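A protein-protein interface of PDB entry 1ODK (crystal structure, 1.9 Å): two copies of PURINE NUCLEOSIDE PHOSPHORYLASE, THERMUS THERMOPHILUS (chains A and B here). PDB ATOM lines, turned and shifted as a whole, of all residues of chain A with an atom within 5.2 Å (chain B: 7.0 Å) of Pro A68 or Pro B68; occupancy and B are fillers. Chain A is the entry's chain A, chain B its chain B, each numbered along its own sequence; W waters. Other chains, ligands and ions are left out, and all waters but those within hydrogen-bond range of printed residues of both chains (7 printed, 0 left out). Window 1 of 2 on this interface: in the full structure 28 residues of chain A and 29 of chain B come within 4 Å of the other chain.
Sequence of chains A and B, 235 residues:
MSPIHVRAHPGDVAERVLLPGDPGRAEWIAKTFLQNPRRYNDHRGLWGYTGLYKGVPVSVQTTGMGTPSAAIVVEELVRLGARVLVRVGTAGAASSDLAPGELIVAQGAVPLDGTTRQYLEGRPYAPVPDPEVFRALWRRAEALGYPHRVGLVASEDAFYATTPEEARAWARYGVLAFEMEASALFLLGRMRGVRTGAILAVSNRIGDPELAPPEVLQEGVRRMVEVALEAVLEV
The backbone NH (N) of Thr A115 lies within hydrogen-bond range of the side-chain carboxylate (OD1) of Asp B157 (3.3 Å). The side-chain carboxylate (OD1) of Asp A157 sits at hydrogen-bond distance from the backbone NH (N) of Thr B115 (3.5 Å).
The side-chain hydroxyl of Thr A67 is in hydrogen-bond range of the side-chain hydroxyl of Thr A115 (2.8 Å). The side-chain hydroxyl (OG1) of Thr A67 lies within hydrogen-bond range of the side-chain carboxylate (OD2) of Asp A157, at 3.5 Å. The side-chain carboxylate (OE1) of Glu B181 sits at hydrogen-bond distance from the backbone NH (N) of Gly B66, 2.9 Å away. N of Thr B67 sits at hydrogen-bond distance from O of Met B180, at 3.0 Å. The side-chain carboxylate (OD1) of Asp B113 is in hydrogen-bond range of the backbone NH (N) of Thr B115. The backbone NH (N) of Gly B114 is in hydrogen-bond range of the side-chain carboxylate (OD1) of Asp B157, at 2.7 Å.
Among the printed residues, merely in contact across the chains: Met A65 with Ser B69, Gly A66 with Pro B68, Pro A68 with Gly B66, Pro A68 with Pro B68, Pro A68 with Asp B157, Pro A68 with Met B180, Ser A69 with Met B65, Ile A72 with Phe B159, Ile A72 with Met B180, Asp A157 with Pro B68, Asp A157 with Gly B114, Asp A157 with Asp B157, Met A180 with Pro B68 and Met A180 with Ile B72.
Of the printed residues of chain B, Met A180 touches Pro B68 (3.7 Å) and Ile B72 (3.9 Å). Of the printed residues of chain A, Gly B66 touches Pro A68 (3.95 Å). Thr A67 touches none of the printed residues of chain B. Thr B63 touches none of the printed residues of chain A. The nearest residue of chain A that does not touch Pro B68 is Met A65 (4.6 Å). The nearest printed residue of chain B that does not touch Met A180 is Ser B69 (5.2 Å).
Of the 20 printed residues of chain B, 10 touch a printed residue of chain A. Printed residues of chain B that touch a printed residue of chain A: Met B65, Gly B66, Pro B68, Ser B69, Ile B72, Gly B114, Thr B115, Asp B157, Phe B159 and Met B180. Hydrophobic or aromatic side chains of chain B within 4 Å of the printed part of chain A: Met B65, Pro B68, Ile B72, Phe B159 and Met B180. Of the 11 printed residues of chain A, 8 touch a printed residue of chain B.
Met A65 touches Ser B69, and with the chains exchanged Ser A69 touches Met B65. Gly A66 touches Pro B68, and with the chains exchanged Pro A68 touches Gly B66. Ile A72 touches Met B180, and with the chains exchanged Met A180 touches Ile B72. Asp B157 touches its own counterpart, Asp A157. Positions printed for both chains: 65, 66, 67, 68, 69, 70, 71, 72, 115, 157 and 180. Of the 16 pairs that touch across the chains among the printed residues, 14 have their exchanged pair printed and touching as well.
Water W4 bridges O of Met A65 (2.6 Å) and O of Met B65 (2.6 Å). Water W7 lies within hydrogen-bond range of O of Asp A157 and O of Pro B68. Water W1 lies within hydrogen-bond range of the side-chain carboxylate (OD2) of Asp A157 (2.7 Å), the side-chain hydroxyl (OG1) of Thr A67 (2.8 Å), the side-chain hydroxyl (OG1) of Thr A115 (2.8 Å) and the side-chain carboxylate (OD1) of Asp B157 (2.8 Å). Water W3 lies within hydrogen-bond range of OD2 of Asp B157 (2.7 Å), OG1 of Thr B115 (2.8 Å), OG1 of Thr B67 (2.8 Å), OD1 of Asp A157 (3.0 Å) and N of Gly B114 (3.2 Å). Water W6 bridges N of Met A65 (2.7 Å) and OG of Ser B69 (2.8 Å). Water W5 lies within hydrogen-bond range of the side-chain hydroxyl (OG) of Ser A69 (2.8 Å) and the backbone NH (N) of Met B65 (2.9 Å).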
ATOM      1  N   MET A  65       9.120   9.028 -17.896  1.00  0.00           N
ATOM      2  CA  MET A  65       7.700   9.005 -17.562  1.00  0.00           C
ATOM      3  C   MET A  65       7.423   8.851 -16.067  1.00  0.00           C
ATOM      4  O   MET A  65       8.039   8.023 -15.401  1.00  0.00           O
ATOM      5  CB  MET A  65       7.007   7.860 -18.308  1.00  0.00           C
ATOM      6  CG  MET A  65       7.212   7.880 -19.815  1.00  0.00           C
ATOM      7  SD  MET A  65       6.308   6.551 -20.635  1.00  0.00           S
ATOM      8  CE  MET A  65       7.341   5.162 -20.241  1.00  0.00           C
ATOM      9  N   GLY A  66       6.483   9.644 -15.554  1.00  0.00           N
ATOM     10  CA  GLY A  66       6.113   9.564 -14.149  1.00  0.00           C
ATOM     11  C   GLY A  66       6.787  10.584 -13.256  1.00  0.00           C
ATOM     12  O   GLY A  66       7.909  11.019 -13.534  1.00  0.00           O
ATOM     13  N   THR A  67       6.111  10.956 -12.171  1.00  0.00           N
ATOM     14  CA  THR A  67       6.660  11.941 -11.242  1.00  0.00           C
ATOM     15  C   THR A  67       7.924  11.475 -10.528  1.00  0.00           C
ATOM     16  O   THR A  67       8.750  12.292 -10.139  1.00  0.00           O
ATOM     17  CB  THR A  67       5.616  12.386 -10.189  1.00  0.00           C
ATOM     18  OG1 THR A  67       4.982  11.239  -9.612  1.00  0.00           O
ATOM     19  CG2 THR A  67       4.571  13.296 -10.830  1.00  0.00           C
ATOM     20  N   PRO A  68       8.095  10.154 -10.340  1.00  0.00           N
ATOM     21  CA  PRO A  68       9.332   9.764  -9.656  1.00  0.00           C
ATOM     22  C   PRO A  68      10.560  10.082 -10.515  1.00  0.00           C
ATOM     23  O   PRO A  68      11.569  10.573 -10.015  1.00  0.00           O
ATOM     24  CB  PRO A  68       9.144   8.264  -9.433  1.00  0.00           C
ATOM     25  CG  PRO A  68       7.658   8.149  -9.239  1.00  0.00           C
ATOM     26  CD  PRO A  68       7.129   9.039 -10.352  1.00  0.00           C
ATOM     27  N   SER A  69      10.458   9.801 -11.810  1.00  0.00           N
ATOM     28  CA  SER A  69      11.553  10.050 -12.744  1.00  0.00           C
ATOM     29  C   SER A  69      11.732  11.556 -12.922  1.00  0.00           C
ATOM     30  O   SER A  69      12.854  12.075 -12.870  1.00  0.00           O
ATOM     31  CB  SER A  69      11.247   9.387 -14.099  1.00  0.00           C
ATOM     32  OG  SER A  69      12.376   9.410 -14.957  1.00  0.00           O
ATOM     33  N   ALA A  70      10.618  12.257 -13.110  1.00  0.00           N
ATOM     34  CA  ALA A  70      10.647  13.710 -13.296  1.00  0.00           C
ATOM     35  C   ALA A  70      11.232  14.430 -12.079  1.00  0.00           C
ATOM     36  O   ALA A  70      12.021  15.362 -12.226  1.00  0.00           O
ATOM     37  CB  ALA A  70       9.232  14.231 -13.583  1.00  0.00           C
ATOM     38  N   ALA A  71      10.840  14.002 -10.876  1.00  0.00           N
ATOM     39  CA  ALA A  71      11.336  14.621  -9.649  1.00  0.00           C
ATOM     40  C   ALA A  71      12.857  14.473  -9.544  1.00  0.00           C
ATOM     41  O   ALA A  71      13.554  15.411  -9.165  1.00  0.00           O
ATOM     42  CB  ALA A  71      10.651  13.996  -8.425  1.00  0.00           C
ATOM     43  N   ILE A  72      13.368  13.293  -9.872  1.00  0.00           N
ATOM     44  CA  ILE A  72      14.808  13.063  -9.835  1.00  0.00           C
ATOM     45  C   ILE A  72      15.482  14.045 -10.791  1.00  0.00           C
ATOM     46  O   ILE A  72      16.447  14.715 -10.434  1.00  0.00           O
ATOM     47  CB  ILE A  72      15.162  11.612 -10.272  1.00  0.00           C
ATOM     48  CG1 ILE A  72      14.890  10.636  -9.123  1.00  0.00           C
ATOM     49  CG2 ILE A  72      16.616  11.531 -10.716  1.00  0.00           C
ATOM     50  CD1 ILE A  72      14.936   9.167  -9.539  1.00  0.00           C
ATOM     51  N   THR A 115       4.591  10.676  -5.615  1.00  0.00           N
ATOM     52  CA  THR A 115       5.823  11.436  -5.419  1.00  0.00           C
ATOM     53  C   THR A 115       5.514  12.688  -4.605  1.00  0.00           C
ATOM     54  O   THR A 115       6.189  12.983  -3.616  1.00  0.00           O
ATOM     55  CB  THR A 115       6.468  11.842  -6.765  1.00  0.00           C
ATOM     56  OG1 THR A 115       6.812  10.665  -7.506  1.00  0.00           O
ATOM     57  CG2 THR A 115       7.729  12.669  -6.528  1.00  0.00           C
ATOM     58  N   ASP A 157      -0.167   8.263 -11.560  1.00  0.00           N
ATOM     59  CA  ASP A 157       0.906   7.276 -11.511  1.00  0.00           C
ATOM     60  C   ASP A 157       0.625   6.031 -12.346  1.00  0.00           C
ATOM     61  O   ASP A 157       1.513   5.527 -13.025  1.00  0.00           O
ATOM     62  CB  ASP A 157       1.141   6.823 -10.065  1.00  0.00           C
ATOM     63  CG  ASP A 157       1.986   7.796  -9.267  1.00  0.00           C
ATOM     64  OD1 ASP A 157       1.999   7.666  -8.024  1.00  0.00           O
ATOM     65  OD2 ASP A 157       2.645   8.676  -9.867  1.00  0.00           O
ATOM     66  N   MET A 180       1.516  12.721 -16.416  1.00  0.00           N
ATOM     67  CA  MET A 180       2.193  12.065 -15.301  1.00  0.00           C
ATOM     68  C   MET A 180       3.429  12.774 -14.749  1.00  0.00           C
ATOM     69  O   MET A 180       4.334  12.114 -14.237  1.00  0.00           O
ATOM     70  CB  MET A 180       2.588  10.645 -15.744  1.00  0.00           C
ATOM     71  CG  MET A 180       1.432   9.830 -16.314  1.00  0.00           C
ATOM     72  SD  MET A 180       1.951   8.273 -17.097  1.00  0.00           S
ATOM     73  CE  MET A 180       2.717   7.442 -15.697  1.00  0.00           C
ATOM     74  N   THR B  63      13.034  -0.425 -18.159  1.00  0.00           N
ATOM     75  CA  THR B  63      11.792  -0.008 -17.500  1.00  0.00           C
ATOM     76  C   THR B  63      11.739   1.493 -17.201  1.00  0.00           C
ATOM     77  O   THR B  63      10.660   2.058 -17.027  1.00  0.00           O
ATOM     78  CB  THR B  63      11.599  -0.696 -16.140  1.00  0.00           C
ATOM     79  OG1 THR B  63      12.613  -0.234 -15.242  1.00  0.00           O
ATOM     80  CG2 THR B  63      11.684  -2.215 -16.268  1.00  0.00           C
ATOM     81  N   MET B  65      12.877   4.738 -14.641  1.00  0.00           N
ATOM     82  CA  MET B  65      12.900   4.829 -13.184  1.00  0.00           C
ATOM     83  C   MET B  65      11.520   5.117 -12.614  1.00  0.00           C
ATOM     84  O   MET B  65      10.778   5.940 -13.155  1.00  0.00           O
ATOM     85  CB  MET B  65      13.853   5.941 -12.734  1.00  0.00           C
ATOM     86  CG  MET B  65      15.256   5.836 -13.309  1.00  0.00           C
ATOM     87  SD  MET B  65      16.289   7.210 -12.764  1.00  0.00           S
ATOM     88  CE  MET B  65      15.731   8.510 -13.821  1.00  0.00           C
ATOM     89  N   GLY B  66      11.186   4.446 -11.515  1.00  0.00           N
ATOM     90  CA  GLY B  66       9.902   4.660 -10.866  1.00  0.00           C
ATOM     91  C   GLY B  66       8.822   3.671 -11.255  1.00  0.00           C
ATOM     92  O   GLY B  66       8.804   3.179 -12.384  1.00  0.00           O
ATOM     93  N   THR B  67       7.917   3.380 -10.322  1.00  0.00           N
ATOM     94  CA  THR B  67       6.831   2.446 -10.585  1.00  0.00           C
ATOM     95  C   THR B  67       5.877   2.882 -11.699  1.00  0.00           C
ATOM     96  O   THR B  67       5.298   2.038 -12.377  1.00  0.00           O
ATOM     97  CB  THR B  67       6.014   2.144  -9.298  1.00  0.00           C
ATOM     98  OG1 THR B  67       5.618   3.368  -8.666  1.00  0.00           O
ATOM     99  CG2 THR B  67       6.848   1.318  -8.323  1.00  0.00           C
ATOM    100  N   PRO B  68       5.693   4.202 -11.908  1.00  0.00           N
ATOM    101  CA  PRO B  68       4.773   4.569 -12.992  1.00  0.00           C
ATOM    102  C   PRO B  68       5.335   4.123 -14.346  1.00  0.00           C
ATOM    103  O   PRO B  68       4.605   3.630 -15.210  1.00  0.00           O
ATOM    104  CB  PRO B  68       4.691   6.096 -12.885  1.00  0.00           C
ATOM    105  CG  PRO B  68       4.927   6.349 -11.420  1.00  0.00           C
ATOM    106  CD  PRO B  68       6.058   5.384 -11.106  1.00  0.00           C
ATOM    107  N   SER B  69       6.640   4.308 -14.519  1.00  0.00           N
ATOM    108  CA  SER B  69       7.303   3.927 -15.759  1.00  0.00           C
ATOM    109  C   SER B  69       7.379   2.408 -15.866  1.00  0.00           C
ATOM    110  O   SER B  69       7.101   1.835 -16.922  1.00  0.00           O
ATOM    111  CB  SER B  69       8.719   4.522 -15.808  1.00  0.00           C
ATOM    112  OG  SER B  69       9.334   4.288 -17.068  1.00  0.00           O
ATOM    113  N   ALA B  70       7.749   1.751 -14.770  1.00  0.00           N
ATOM    114  CA  ALA B  70       7.868   0.297 -14.774  1.00  0.00           C
ATOM    115  C   ALA B  70       6.521  -0.377 -15.005  1.00  0.00           C
ATOM    116  O   ALA B  70       6.450  -1.402 -15.683  1.00  0.00           O
ATOM    117  CB  ALA B  70       8.482  -0.188 -13.459  1.00  0.00           C
ATOM    118  N   ALA B  71       5.455   0.198 -14.451  1.00  0.00           N
ATOM    119  CA  ALA B  71       4.122  -0.384 -14.606  1.00  0.00           C
ATOM    120  C   ALA B  71       3.683  -0.344 -16.059  1.00  0.00           C
ATOM    121  O   ALA B  71       3.108  -1.308 -16.567  1.00  0.00           O
ATOM    122  CB  ALA B  71       3.104   0.352 -13.722  1.00  0.00           C
ATOM    123  N   ILE B  72       3.952   0.771 -16.726  1.00  0.00           N
ATOM    124  CA  ILE B  72       3.596   0.907 -18.133  1.00  0.00           C
ATOM    125  C   ILE B  72       4.325  -0.156 -18.955  1.00  0.00           C
ATOM    126  O   ILE B  72       3.736  -0.786 -19.833  1.00  0.00           O
ATOM    127  CB  ILE B  72       3.986   2.300 -18.664  1.00  0.00           C
ATOM    128  CG1 ILE B  72       2.949   3.332 -18.214  1.00  0.00           C
ATOM    129  CG2 ILE B  72       4.132   2.265 -20.194  1.00  0.00           C
ATOM    130  CD1 ILE B  72       3.372   4.772 -18.470  1.00  0.00           C
ATOM    131  N   VAL B  73       5.611  -0.343 -18.668  1.00  0.00           N
ATOM    132  CA  VAL B  73       6.420  -1.316 -19.397  1.00  0.00           C
ATOM    133  C   VAL B  73       5.978  -2.750 -19.110  1.00  0.00           C
ATOM    134  O   VAL B  73       5.873  -3.570 -20.028  1.00  0.00           O
ATOM    135  CB  VAL B  73       7.924  -1.146 -19.062  1.00  0.00           C
ATOM    136  CG1 VAL B  73       8.750  -2.249 -19.735  1.00  0.00           C
ATOM    137  CG2 VAL B  73       8.403   0.214 -19.537  1.00  0.00           C
ATOM    138  N   ASP B 113       4.974   3.629  -2.821  1.00  0.00           N
ATOM    139  CA  ASP B 113       4.719   4.292  -4.099  1.00  0.00           C
ATOM    140  C   ASP B 113       3.234   4.512  -4.407  1.00  0.00           C
ATOM    141  O   ASP B 113       2.368   3.779  -3.924  1.00  0.00           O
ATOM    142  CB  ASP B 113       5.331   3.461  -5.224  1.00  0.00           C
ATOM    143  CG  ASP B 113       4.572   2.177  -5.461  1.00  0.00           C
ATOM    144  OD1 ASP B 113       4.040   2.010  -6.578  1.00  0.00           O
ATOM    145  OD2 ASP B 113       4.498   1.344  -4.531  1.00  0.00           O
ATOM    146  N   GLY B 114       2.952   5.506  -5.246  1.00  0.00           N
ATOM    147  CA  GLY B 114       1.575   5.808  -5.601  1.00  0.00           C
ATOM    148  C   GLY B 114       0.983   4.970  -6.722  1.00  0.00           C
ATOM    149  O   GLY B 114      -0.229   4.974  -6.928  1.00  0.00           O
ATOM    150  N   THR B 115       1.824   4.258  -7.465  1.00  0.00           N
ATOM    151  CA  THR B 115       1.317   3.429  -8.547  1.00  0.00           C
ATOM    152  C   THR B 115       0.563   2.231  -7.977  1.00  0.00           C
ATOM    153  O   THR B 115      -0.552   1.935  -8.403  1.00  0.00           O
ATOM    154  CB  THR B 115       2.459   2.936  -9.471  1.00  0.00           C
ATOM    155  OG1 THR B 115       3.127   4.069 -10.036  1.00  0.00           O
ATOM    156  CG2 THR B 115       1.902   2.077 -10.606  1.00  0.00           C
ATOM    157  N   GLU B 156       9.999   3.239  -3.339  1.00  0.00           N
ATOM    158  CA  GLU B 156       9.552   4.607  -3.088  1.00  0.00           C
ATOM    159  C   GLU B 156       9.419   5.428  -4.364  1.00  0.00           C
ATOM    160  O   GLU B 156       9.900   5.025  -5.427  1.00  0.00           O
ATOM    161  CB  GLU B 156      10.538   5.299  -2.151  1.00  0.00           C
ATOM    162  CG  GLU B 156      11.932   5.371  -2.726  1.00  0.00           C
ATOM    163  CD  GLU B 156      12.885   6.135  -1.847  1.00  0.00           C
ATOM    164  OE1 GLU B 156      14.086   6.172  -2.175  1.00  0.00           O
ATOM    165  OE2 GLU B 156      12.428   6.701  -0.832  1.00  0.00           O
ATOM    166  N   ASP B 157       8.779   6.589  -4.238  1.00  0.00           N
ATOM    167  CA  ASP B 157       8.556   7.510  -5.354  1.00  0.00           C
ATOM    168  C   ASP B 157       9.518   8.694  -5.358  1.00  0.00           C
ATOM    169  O   ASP B 157       9.996   9.106  -6.415  1.00  0.00           O
ATOM    170  CB  ASP B 157       7.127   8.071  -5.307  1.00  0.00           C
ATOM    171  CG  ASP B 157       6.098   7.127  -5.898  1.00  0.00           C
ATOM    172  OD1 ASP B 157       4.891   7.375  -5.695  1.00  0.00           O
ATOM    173  OD2 ASP B 157       6.487   6.149  -6.570  1.00  0.00           O
ATOM    174  N   ALA B 158       9.787   9.248  -4.176  1.00  0.00           N
ATOM    175  CA  ALA B 158      10.660  10.419  -4.051  1.00  0.00           C
ATOM    176  C   ALA B 158      12.083  10.111  -3.590  1.00  0.00           C
ATOM    177  O   ALA B 158      12.403  10.194  -2.402  1.00  0.00           O
ATOM    178  CB  ALA B 158      10.016  11.447  -3.114  1.00  0.00           C
ATOM    179  N   PHE B 159      12.930   9.773  -4.558  1.00  0.00           N
ATOM    180  CA  PHE B 159      14.336   9.444  -4.336  1.00  0.00           C
ATOM    181  C   PHE B 159      15.032  10.424  -3.386  1.00  0.00           C
ATOM    182  O   PHE B 159      15.734  10.018  -2.460  1.00  0.00           O
ATOM    183  CB  PHE B 159      15.055   9.450  -5.693  1.00  0.00           C
ATOM    184  CG  PHE B 159      16.488   8.996  -5.638  1.00  0.00           C
ATOM    185  CD1 PHE B 159      16.810   7.644  -5.717  1.00  0.00           C
ATOM    186  CD2 PHE B 159      17.520   9.922  -5.522  1.00  0.00           C
ATOM    187  CE1 PHE B 159      18.142   7.222  -5.684  1.00  0.00           C
ATOM    188  CE2 PHE B 159      18.858   9.509  -5.486  1.00  0.00           C
ATOM    189  CZ  PHE B 159      19.169   8.160  -5.567  1.00  0.00           C
ATOM    190  N   MET B 180      13.011   1.633  -6.613  1.00  0.00           N
ATOM    191  CA  MET B 180      11.800   2.318  -7.068  1.00  0.00           C
ATOM    192  C   MET B 180      10.935   1.586  -8.088  1.00  0.00           C
ATOM    193  O   MET B 180      10.253   2.231  -8.887  1.00  0.00           O
ATOM    194  CB  MET B 180      12.204   3.681  -7.655  1.00  0.00           C
ATOM    195  CG  MET B 180      13.025   4.563  -6.705  1.00  0.00           C
ATOM    196  SD  MET B 180      13.717   6.042  -7.511  1.00  0.00           S
ATOM    197  CE  MET B 180      12.207   6.957  -7.833  1.00  0.00           C
ATOM    198  N   GLU B 181      10.928   0.259  -8.069  1.00  0.00           N
ATOM    199  CA  GLU B 181      10.141  -0.459  -9.067  1.00  0.00           C
ATOM    200  C   GLU B 181       9.473  -1.756  -8.620  1.00  0.00           C
ATOM    201  O   GLU B 181       8.397  -2.108  -9.109  1.00  0.00           O
ATOM    202  CB  GLU B 181      11.027  -0.773 -10.282  1.00  0.00           C
ATOM    203  CG  GLU B 181      11.503   0.440 -11.081  1.00  0.00           C
ATOM    204  CD  GLU B 181      12.698   1.160 -10.473  1.00  0.00           C
ATOM    205  OE1 GLU B 181      13.026   2.255 -10.975  1.00  0.00           O
ATOM    206  OE2 GLU B 181      13.317   0.645  -9.511  1.00  0.00           O
ATOM    207  N   ALA B 184       5.382  -2.402  -7.735  1.00  0.00           N
ATOM    208  CA  ALA B 184       4.461  -2.440  -8.877  1.00  0.00           C
ATOM    209  C   ALA B 184       4.600  -3.719  -9.698  1.00  0.00           C
ATOM    210  O   ALA B 184       3.608  -4.292 -10.152  1.00  0.00           O
ATOM    211  CB  ALA B 184       4.679  -1.210  -9.780  1.00  0.00           C
HETATM  212  O   HOH W   1       4.569   9.003  -7.998  1.00  0.00           O
HETATM  213  O   HOH W   2      11.852  10.652  -7.301  1.00  0.00           O
HETATM  214  O   HOH W   3       4.282   5.781  -8.144  1.00  0.00           O
HETATM  215  O   HOH W   4       8.420   7.066 -13.044  1.00  0.00           O
HETATM  216  O   HOH W   5      12.892   7.061 -16.331  1.00  0.00           O
HETATM  217  O   HOH W   6      10.485   6.644 -17.940  1.00  0.00           O
HETATM  218  O   HOH W   7       1.890   3.653 -14.893  1.00  0.00           O
